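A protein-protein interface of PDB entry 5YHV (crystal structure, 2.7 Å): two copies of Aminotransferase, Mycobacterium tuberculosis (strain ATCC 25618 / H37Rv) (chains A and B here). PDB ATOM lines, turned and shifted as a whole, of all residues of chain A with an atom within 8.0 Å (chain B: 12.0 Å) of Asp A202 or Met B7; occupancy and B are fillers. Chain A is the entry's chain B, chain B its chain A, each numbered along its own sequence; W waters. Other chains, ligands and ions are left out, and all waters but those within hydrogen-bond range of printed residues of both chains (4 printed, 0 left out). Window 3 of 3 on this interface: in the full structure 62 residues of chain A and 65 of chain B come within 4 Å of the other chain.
Water W4 lies within hydrogen-bond range of the side-chain amide oxygen (OD1) of Asn A231 (2.7 Å), the side-chain carboxylate (OD2) of Asp B9 (2.8 Å) and the guanidinium group (NH1) of Arg A204 (3.3 Å). Water W1 lies within hydrogen-bond range of NE of Arg A204 (2.8 Å) and O of Arg B10 (2.9 Å). Water W2 lies within hydrogen-bond range of the side-chain carboxylate of Asp B9 (2.9 Å), the backbone NH of Arg B10 (3.3 Å) and the side-chain carboxylate of Asp A202 (3.4 Å). Water W3 lies within hydrogen-bond range of the side-chain carboxylate of Asp B9 and the side-chain amide oxygen of Asn A231.
Of the 15 printed residues of chain A, 4 touch a printed residue of chain B. Hydrophobic or aromatic side chains of chain B that line the printed part of chain A: Met B7 and Ala B12. Among the printed residues, 7 pairs touch across the chains. Among the printed residues, Asp or Glu carboxylates within 4 Å of a Lys or Arg side-chain nitrogen of the other chain: Asp A202 with Arg B10 (3.1 Å) and Arg A204 with Asp B9 (3.2 Å).
Asp A202 touches just these residues of chain B: Met B7 (3.5 Å), Thr B8 (3.4 Å) and Arg B10 (2.8 Å). Of chain A, only Asp A202 comes within 4 Å of Met B7. Arg A171 touches just one residue of chain B: Arg B10. No residue of chain B comes within 4 Å of Cys A198. No residue of chain B comes within 4 Å of Ser A201. No residue of chain B comes within 4 Å of Val A203. Arg A204 touches just these residues of chain B: Asp B9 and Arg B10. Printed residues of chain A within 4 Å of Arg B10: Arg A171, Asp A202 and Arg A204. Printed residues of chain A within 4 Å of Thr B8: Asp A202 (3.4 Å). The nearest residue of chain B that does not touch Asp A202 is Asp B9 (5.0 Å). The nearest printed residue of chain A that does not touch Ala B12 is Arg A204 (7.1 Å).
O of Arg A171 lies within hydrogen-bond range of N of Arg A204 (2.9 Å). O of Asn A231 is in hydrogen-bond range of NH1 of Arg A204 (2.7 Å).
No position is printed for both chains. Of the 7 pairs that touch across the chains among the printed residues, none has its exchanged pair printed and touching as well.
Among the printed residues, pairs that only touch across the chains: Phe A118 with Ala B12, Arg A171 with Arg B10 and Asp A202 with Met B7.
OD1 of Asp B9 lies within salt-bridge range of NH2 of Arg A204, at 3.2 Å. The guanidinium group (NH1) of Arg B10 is in salt-bridge range of the side-chain carboxylate (OD2) of Asp A202, at 3.1 Å. The backbone carbonyl oxygen of Arg B10 is in hydrogen-bond range of the guanidinium group of Arg A204, at 2.8 Å. The side-chain carboxylate (OD2) of Asp A202 sits close to the backbone carbonyl oxygen (O) of Thr B8, 3.4 Å away.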
ATOM      1  N   PHE A 118      20.585 -11.494 -17.495  1.00  0.00           N
ATOM      2  CA  PHE A 118      19.342 -10.778 -17.210  1.00  0.00           C
ATOM      3  C   PHE A 118      19.541  -9.315 -16.846  1.00  0.00           C
ATOM      4  O   PHE A 118      20.491  -8.962 -16.142  1.00  0.00           O
ATOM      5  CB  PHE A 118      18.536 -11.492 -16.111  1.00  0.00           C
ATOM      6  CG  PHE A 118      18.469 -12.987 -16.272  1.00  0.00           C
ATOM      7  CD1 PHE A 118      17.890 -13.564 -17.413  1.00  0.00           C
ATOM      8  CD2 PHE A 118      18.983 -13.827 -15.285  1.00  0.00           C
ATOM      9  CE1 PHE A 118      17.841 -14.942 -17.561  1.00  0.00           C
ATOM     10  CE2 PHE A 118      18.924 -15.211 -15.429  1.00  0.00           C
ATOM     11  CZ  PHE A 118      18.353 -15.766 -16.567  1.00  0.00           C
ATOM     12  N   LEU A 170       8.625 -15.675 -19.747  1.00  0.00           N
ATOM     13  CA  LEU A 170       9.824 -15.653 -18.913  1.00  0.00           C
ATOM     14  C   LEU A 170      11.047 -15.275 -19.743  1.00  0.00           C
ATOM     15  O   LEU A 170      11.086 -15.517 -20.952  1.00  0.00           O
ATOM     16  CB  LEU A 170      10.053 -17.021 -18.256  1.00  0.00           C
ATOM     17  CG  LEU A 170       8.963 -17.689 -17.412  1.00  0.00           C
ATOM     18  CD1 LEU A 170       9.193 -19.191 -17.331  1.00  0.00           C
ATOM     19  CD2 LEU A 170       8.864 -17.070 -16.028  1.00  0.00           C
ATOM     20  N   ARG A 171      12.040 -14.681 -19.084  1.00  0.00           N
ATOM     21  CA  ARG A 171      13.356 -14.437 -19.685  1.00  0.00           C
ATOM     22  C   ARG A 171      14.365 -15.507 -19.270  1.00  0.00           C
ATOM     23  O   ARG A 171      15.297 -15.816 -20.023  1.00  0.00           O
ATOM     24  CB  ARG A 171      13.877 -13.041 -19.332  1.00  0.00           C
ATOM     25  CG  ARG A 171      13.170 -11.892 -20.042  1.00  0.00           C
ATOM     26  CD  ARG A 171      13.519 -11.808 -21.526  1.00  0.00           C
ATOM     27  NE  ARG A 171      12.446 -11.204 -22.321  1.00  0.00           N
ATOM     28  CZ  ARG A 171      12.485  -9.991 -22.883  1.00  0.00           C
ATOM     29  NH1 ARG A 171      13.554  -9.209 -22.756  1.00  0.00           N
ATOM     30  NH2 ARG A 171      11.442  -9.562 -23.583  1.00  0.00           N
ATOM     31  N   GLY A 172      14.163 -16.077 -18.078  1.00  0.00           N
ATOM     32  CA  GLY A 172      15.053 -17.098 -17.527  1.00  0.00           C
ATOM     33  C   GLY A 172      14.402 -18.197 -16.714  1.00  0.00           C
ATOM     34  O   GLY A 172      13.333 -18.001 -16.141  1.00  0.00           O
ATOM     35  N   SER A 196      15.267 -27.907 -24.354  1.00  0.00           N
ATOM     36  CA  SER A 196      14.734 -27.694 -25.703  1.00  0.00           C
ATOM     37  C   SER A 196      13.674 -26.594 -25.732  1.00  0.00           C
ATOM     38  O   SER A 196      13.715 -25.717 -26.608  1.00  0.00           O
ATOM     39  CB  SER A 196      14.172 -28.993 -26.284  1.00  0.00           C
ATOM     40  OG  SER A 196      15.222 -29.875 -26.638  1.00  0.00           O
ATOM     41  N   TRP A 197      12.755 -26.637 -24.764  1.00  0.00           N
ATOM     42  CA  TRP A 197      11.711 -25.628 -24.617  1.00  0.00           C
ATOM     43  C   TRP A 197      12.304 -24.221 -24.549  1.00  0.00           C
ATOM     44  O   TRP A 197      11.865 -23.324 -25.268  1.00  0.00           O
ATOM     45  CB  TRP A 197      10.843 -25.905 -23.378  1.00  0.00           C
ATOM     46  CG  TRP A 197       9.767 -24.868 -23.172  1.00  0.00           C
ATOM     47  CD1 TRP A 197       8.539 -24.813 -23.775  1.00  0.00           C
ATOM     48  CD2 TRP A 197       9.874 -23.673 -22.383  1.00  0.00           C
ATOM     49  NE1 TRP A 197       7.885 -23.673 -23.405  1.00  0.00           N
ATOM     50  CE2 TRP A 197       8.669 -22.960 -22.539  1.00  0.00           C
ATOM     51  CE3 TRP A 197      10.896 -23.119 -21.594  1.00  0.00           C
ATOM     52  CZ2 TRP A 197       8.425 -21.742 -21.894  1.00  0.00           C
ATOM     53  CZ3 TRP A 197      10.651 -21.922 -20.927  1.00  0.00           C
ATOM     54  CH2 TRP A 197       9.432 -21.236 -21.094  1.00  0.00           C
ATOM     55  N   CYS A 198      13.303 -24.066 -23.684  1.00  0.00           N
ATOM     56  CA  CYS A 198      14.002 -22.803 -23.460  1.00  0.00           C
ATOM     57  C   CYS A 198      14.551 -22.191 -24.754  1.00  0.00           C
ATOM     58  O   CYS A 198      14.316 -21.011 -25.027  1.00  0.00           O
ATOM     59  CB  CYS A 198      15.110 -22.996 -22.424  1.00  0.00           C
ATOM     60  SG  CYS A 198      14.507 -23.012 -20.713  1.00  0.00           S
ATOM     61  N   ASP A 199      15.253 -23.008 -25.549  1.00  0.00           N
ATOM     62  CA  ASP A 199      15.770 -22.602 -26.857  1.00  0.00           C
ATOM     63  C   ASP A 199      14.659 -22.067 -27.759  1.00  0.00           C
ATOM     64  O   ASP A 199      14.767 -20.954 -28.289  1.00  0.00           O
ATOM     65  CB  ASP A 199      16.479 -23.768 -27.540  1.00  0.00           C
ATOM     66  CG  ASP A 199      17.791 -24.134 -26.878  1.00  0.00           C
ATOM     67  OD1 ASP A 199      18.273 -23.444 -25.951  1.00  0.00           O
ATOM     68  OD2 ASP A 199      18.383 -25.125 -27.346  1.00  0.00           O
ATOM     69  N   ALA A 200      13.592 -22.857 -27.890  1.00  0.00           N
ATOM     70  CA  ALA A 200      12.437 -22.515 -28.716  1.00  0.00           C
ATOM     71  C   ALA A 200      11.748 -21.232 -28.254  1.00  0.00           C
ATOM     72  O   ALA A 200      11.327 -20.421 -29.078  1.00  0.00           O
ATOM     73  CB  ALA A 200      11.452 -23.671 -28.739  1.00  0.00           C
ATOM     74  N   SER A 201      11.669 -21.052 -26.936  1.00  0.00           N
ATOM     75  CA  SER A 201      10.971 -19.923 -26.327  1.00  0.00           C
ATOM     76  C   SER A 201      11.869 -18.693 -26.130  1.00  0.00           C
ATOM     77  O   SER A 201      11.406 -17.669 -25.607  1.00  0.00           O
ATOM     78  CB  SER A 201      10.332 -20.351 -25.002  1.00  0.00           C
ATOM     79  OG  SER A 201       9.803 -21.656 -25.093  1.00  0.00           O
ATOM     80  N   ASP A 202      13.134 -18.800 -26.556  1.00  0.00           N
ATOM     81  CA  ASP A 202      14.170 -17.761 -26.354  1.00  0.00           C
ATOM     82  C   ASP A 202      14.336 -17.366 -24.864  1.00  0.00           C
ATOM     83  O   ASP A 202      14.456 -16.186 -24.506  1.00  0.00           O
ATOM     84  CB  ASP A 202      13.919 -16.540 -27.266  1.00  0.00           C
ATOM     85  CG  ASP A 202      15.189 -15.735 -27.563  1.00  0.00           C
ATOM     86  OD1 ASP A 202      16.224 -16.301 -28.000  1.00  0.00           O
ATOM     87  OD2 ASP A 202      15.137 -14.509 -27.343  1.00  0.00           O
ATOM     88  N   VAL A 203      14.335 -18.387 -24.012  1.00  0.00           N
ATOM     89  CA  VAL A 203      14.469 -18.239 -22.560  1.00  0.00           C
ATOM     90  C   VAL A 203      15.824 -18.814 -22.145  1.00  0.00           C
ATOM     91  O   VAL A 203      16.205 -19.892 -22.591  1.00  0.00           O
ATOM     92  CB  VAL A 203      13.311 -18.951 -21.812  1.00  0.00           C
ATOM     93  CG1 VAL A 203      13.478 -18.881 -20.309  1.00  0.00           C
ATOM     94  CG2 VAL A 203      11.975 -18.352 -22.203  1.00  0.00           C
ATOM     95  N   ARG A 204      16.551 -18.084 -21.304  1.00  0.00           N
ATOM     96  CA  ARG A 204      17.863 -18.535 -20.840  1.00  0.00           C
ATOM     97  C   ARG A 204      17.735 -19.562 -19.713  1.00  0.00           C
ATOM     98  O   ARG A 204      17.049 -19.316 -18.718  1.00  0.00           O
ATOM     99  CB  ARG A 204      18.713 -17.343 -20.395  1.00  0.00           C
ATOM    100  CG  ARG A 204      20.161 -17.683 -20.062  1.00  0.00           C
ATOM    101  CD  ARG A 204      20.974 -18.057 -21.290  1.00  0.00           C
ATOM    102  NE  ARG A 204      21.190 -16.915 -22.184  1.00  0.00           N
ATOM    103  CZ  ARG A 204      21.817 -16.972 -23.360  1.00  0.00           C
ATOM    104  NH1 ARG A 204      22.309 -18.114 -23.819  1.00  0.00           N
ATOM    105  NH2 ARG A 204      21.953 -15.872 -24.084  1.00  0.00           N
ATOM    106  N   LEU A 205      18.401 -20.708 -19.873  1.00  0.00           N
ATOM    107  CA  LEU A 205      18.411 -21.737 -18.836  1.00  0.00           C
ATOM    108  C   LEU A 205      19.680 -21.694 -17.983  1.00  0.00           C
ATOM    109  O   LEU A 205      20.799 -21.715 -18.504  1.00  0.00           O
ATOM    110  CB  LEU A 205      18.184 -23.141 -19.411  1.00  0.00           C
ATOM    111  CG  LEU A 205      18.321 -24.351 -18.454  1.00  0.00           C
ATOM    112  CD1 LEU A 205      17.260 -24.340 -17.362  1.00  0.00           C
ATOM    113  CD2 LEU A 205      18.297 -25.675 -19.193  1.00  0.00           C
ATOM    114  N   ASN A 231      23.132 -23.408 -25.222  1.00  0.00           N
ATOM    115  CA  ASN A 231      22.628 -22.068 -24.930  1.00  0.00           C
ATOM    116  C   ASN A 231      22.465 -21.850 -23.434  1.00  0.00           C
ATOM    117  O   ASN A 231      22.482 -20.716 -22.969  1.00  0.00           O
ATOM    118  CB  ASN A 231      21.304 -21.810 -25.655  1.00  0.00           C
ATOM    119  CG  ASN A 231      21.449 -21.821 -27.164  1.00  0.00           C
ATOM    120  OD1 ASN A 231      22.159 -20.991 -27.734  1.00  0.00           O
ATOM    121  ND2 ASN A 231      20.784 -22.771 -27.820  1.00  0.00           N
ATOM    122  N   HIS B   3      15.700 -22.519 -44.546  1.00  0.00           N
ATOM    123  CA  HIS B   3      16.354 -21.569 -43.660  1.00  0.00           C
ATOM    124  C   HIS B   3      15.294 -20.749 -42.939  1.00  0.00           C
ATOM    125  O   HIS B   3      14.149 -20.664 -43.394  1.00  0.00           O
ATOM    126  CB  HIS B   3      17.280 -20.661 -44.463  1.00  0.00           C
ATOM    127  CG  HIS B   3      18.474 -21.365 -45.025  1.00  0.00           C
ATOM    128  ND1 HIS B   3      18.430 -22.083 -46.201  1.00  0.00           N
ATOM    129  CD2 HIS B   3      19.746 -21.464 -44.570  1.00  0.00           C
ATOM    130  CE1 HIS B   3      19.624 -22.592 -46.447  1.00  0.00           C
ATOM    131  NE2 HIS B   3      20.440 -22.232 -45.473  1.00  0.00           N
ATOM    132  N   HIS B   4      15.673 -20.169 -41.803  1.00  0.00           N
ATOM    133  CA  HIS B   4      14.786 -19.301 -41.030  1.00  0.00           C
ATOM    134  C   HIS B   4      15.570 -18.384 -40.101  1.00  0.00           C
ATOM    135  O   HIS B   4      16.666 -18.731 -39.656  1.00  0.00           O
ATOM    136  CB  HIS B   4      13.778 -20.125 -40.217  1.00  0.00           C
ATOM    137  CG  HIS B   4      12.699 -19.302 -39.584  1.00  0.00           C
ATOM    138  ND1 HIS B   4      12.540 -19.205 -38.218  1.00  0.00           N
ATOM    139  CD2 HIS B   4      11.742 -18.515 -40.131  1.00  0.00           C
ATOM    140  CE1 HIS B   4      11.522 -18.408 -37.951  1.00  0.00           C
ATOM    141  NE2 HIS B   4      11.017 -17.978 -39.094  1.00  0.00           N
ATOM    142  N   HIS B   5      14.991 -17.217 -39.824  1.00  0.00           N
ATOM    143  CA  HIS B   5      15.478 -16.277 -38.816  1.00  0.00           C
ATOM    144  C   HIS B   5      15.717 -16.977 -37.478  1.00  0.00           C
ATOM    145  O   HIS B   5      14.896 -17.784 -37.032  1.00  0.00           O
ATOM    146  CB  HIS B   5      14.470 -15.126 -38.673  1.00  0.00           C
ATOM    147  CG  HIS B   5      14.632 -14.301 -37.432  1.00  0.00           C
ATOM    148  ND1 HIS B   5      13.981 -14.598 -36.254  1.00  0.00           N
ATOM    149  CD2 HIS B   5      15.343 -13.176 -37.191  1.00  0.00           C
ATOM    150  CE1 HIS B   5      14.296 -13.699 -35.339  1.00  0.00           C
ATOM    151  NE2 HIS B   5      15.120 -12.824 -35.883  1.00  0.00           N
ATOM    152  N   HIS B   6      16.860 -16.681 -36.867  1.00  0.00           N
ATOM    153  CA  HIS B   6      17.179 -17.166 -35.528  1.00  0.00           C
ATOM    154  C   HIS B   6      16.933 -16.035 -34.554  1.00  0.00           C
ATOM    155  O   HIS B   6      17.334 -14.892 -34.812  1.00  0.00           O
ATOM    156  CB  HIS B   6      18.627 -17.667 -35.431  1.00  0.00           C
ATOM    157  CG  HIS B   6      18.962 -18.762 -36.401  1.00  0.00           C
ATOM    158  ND1 HIS B   6      20.245 -18.979 -36.863  1.00  0.00           N
ATOM    159  CD2 HIS B   6      18.182 -19.692 -37.007  1.00  0.00           C
ATOM    160  CE1 HIS B   6      20.241 -20.000 -37.704  1.00  0.00           C
ATOM    161  NE2 HIS B   6      19.003 -20.449 -37.810  1.00  0.00           N
ATOM    162  N   MET B   7      16.249 -16.356 -33.458  1.00  0.00           N
ATOM    163  CA  MET B   7      15.940 -15.387 -32.407  1.00  0.00           C
ATOM    164  C   MET B   7      17.221 -14.790 -31.853  1.00  0.00           C
ATOM    165  O   MET B   7      18.194 -15.518 -31.620  1.00  0.00           O
ATOM    166  CB  MET B   7      15.122 -16.036 -31.285  1.00  0.00           C
ATOM    167  CG  MET B   7      13.613 -15.939 -31.467  1.00  0.00           C
ATOM    168  SD  MET B   7      13.018 -14.237 -31.361  1.00  0.00           S
ATOM    169  CE  MET B   7      11.250 -14.476 -31.516  1.00  0.00           C
ATOM    170  N   THR B   8      17.223 -13.465 -31.683  1.00  0.00           N
ATOM    171  CA  THR B   8      18.394 -12.748 -31.162  1.00  0.00           C
ATOM    172  C   THR B   8      18.831 -13.365 -29.830  1.00  0.00           C
ATOM    173  O   THR B   8      18.022 -13.510 -28.899  1.00  0.00           O
ATOM    174  CB  THR B   8      18.154 -11.219 -31.059  1.00  0.00           C
ATOM    175  OG1 THR B   8      18.012 -10.667 -32.376  1.00  0.00           O
ATOM    176  CG2 THR B   8      19.323 -10.508 -30.363  1.00  0.00           C
ATOM    177  N   ASP B   9      20.108 -13.767 -29.786  1.00  0.00           N
ATOM    178  CA  ASP B   9      20.738 -14.321 -28.583  1.00  0.00           C
ATOM    179  C   ASP B   9      20.973 -13.183 -27.577  1.00  0.00           C
ATOM    180  O   ASP B   9      21.702 -12.230 -27.886  1.00  0.00           O
ATOM    181  CB  ASP B   9      22.064 -14.994 -28.965  1.00  0.00           C
ATOM    182  CG  ASP B   9      22.311 -16.306 -28.224  1.00  0.00           C
ATOM    183  OD1 ASP B   9      21.669 -16.571 -27.181  1.00  0.00           O
ATOM    184  OD2 ASP B   9      23.172 -17.075 -28.692  1.00  0.00           O
ATOM    185  N   ARG B  10      20.346 -13.282 -26.401  1.00  0.00           N
ATOM    186  CA  ARG B  10      20.279 -12.165 -25.464  1.00  0.00           C
ATOM    187  C   ARG B  10      21.454 -12.104 -24.493  1.00  0.00           C
ATOM    188  O   ARG B  10      21.787 -13.079 -23.834  1.00  0.00           O
ATOM    189  CB  ARG B  10      18.945 -12.163 -24.699  1.00  0.00           C
ATOM    190  CG  ARG B  10      17.814 -11.453 -25.419  1.00  0.00           C
ATOM    191  CD  ARG B  10      16.747 -11.006 -24.432  1.00  0.00           C
ATOM    192  NE  ARG B  10      15.400 -11.216 -24.961  1.00  0.00           N
ATOM    193  CZ  ARG B  10      14.743 -12.379 -24.948  1.00  0.00           C
ATOM    194  NH1 ARG B  10      15.298 -13.476 -24.438  1.00  0.00           N
ATOM    195  NH2 ARG B  10      13.521 -12.450 -25.455  1.00  0.00           N
ATOM    196  N   VAL B  11      22.081 -10.930 -24.445  1.00  0.00           N
ATOM    197  CA  VAL B  11      23.079 -10.553 -23.449  1.00  0.00           C
ATOM    198  C   VAL B  11      22.501  -9.315 -22.763  1.00  0.00           C
ATOM    199  O   VAL B  11      21.980  -8.408 -23.441  1.00  0.00           O
ATOM    200  CB  VAL B  11      24.451 -10.216 -24.096  1.00  0.00           C
ATOM    201  CG1 VAL B  11      25.480  -9.794 -23.046  1.00  0.00           C
ATOM    202  CG2 VAL B  11      24.982 -11.391 -24.909  1.00  0.00           C
ATOM    203  N   ALA B  12      22.578  -9.279 -21.430  1.00  0.00           N
ATOM    204  CA  ALA B  12      22.075  -8.149 -20.648  1.00  0.00           C
ATOM    205  C   ALA B  12      22.807  -6.855 -21.000  1.00  0.00           C
ATOM    206  O   ALA B  12      24.015  -6.872 -21.272  1.00  0.00           O
ATOM    207  CB  ALA B  12      22.193  -8.439 -19.164  1.00  0.00           C
HETATM  208  O   HOH W   1      20.514 -14.276 -21.554  1.00  0.00           O
HETATM  209  O   HOH W   2      19.004 -16.283 -26.029  1.00  0.00           O
HETATM  210  O   HOH W   3      19.825 -18.913 -26.780  1.00  0.00           O
HETATM  211  O   HOH W   4      23.737 -18.999 -26.712  1.00  0.00           O
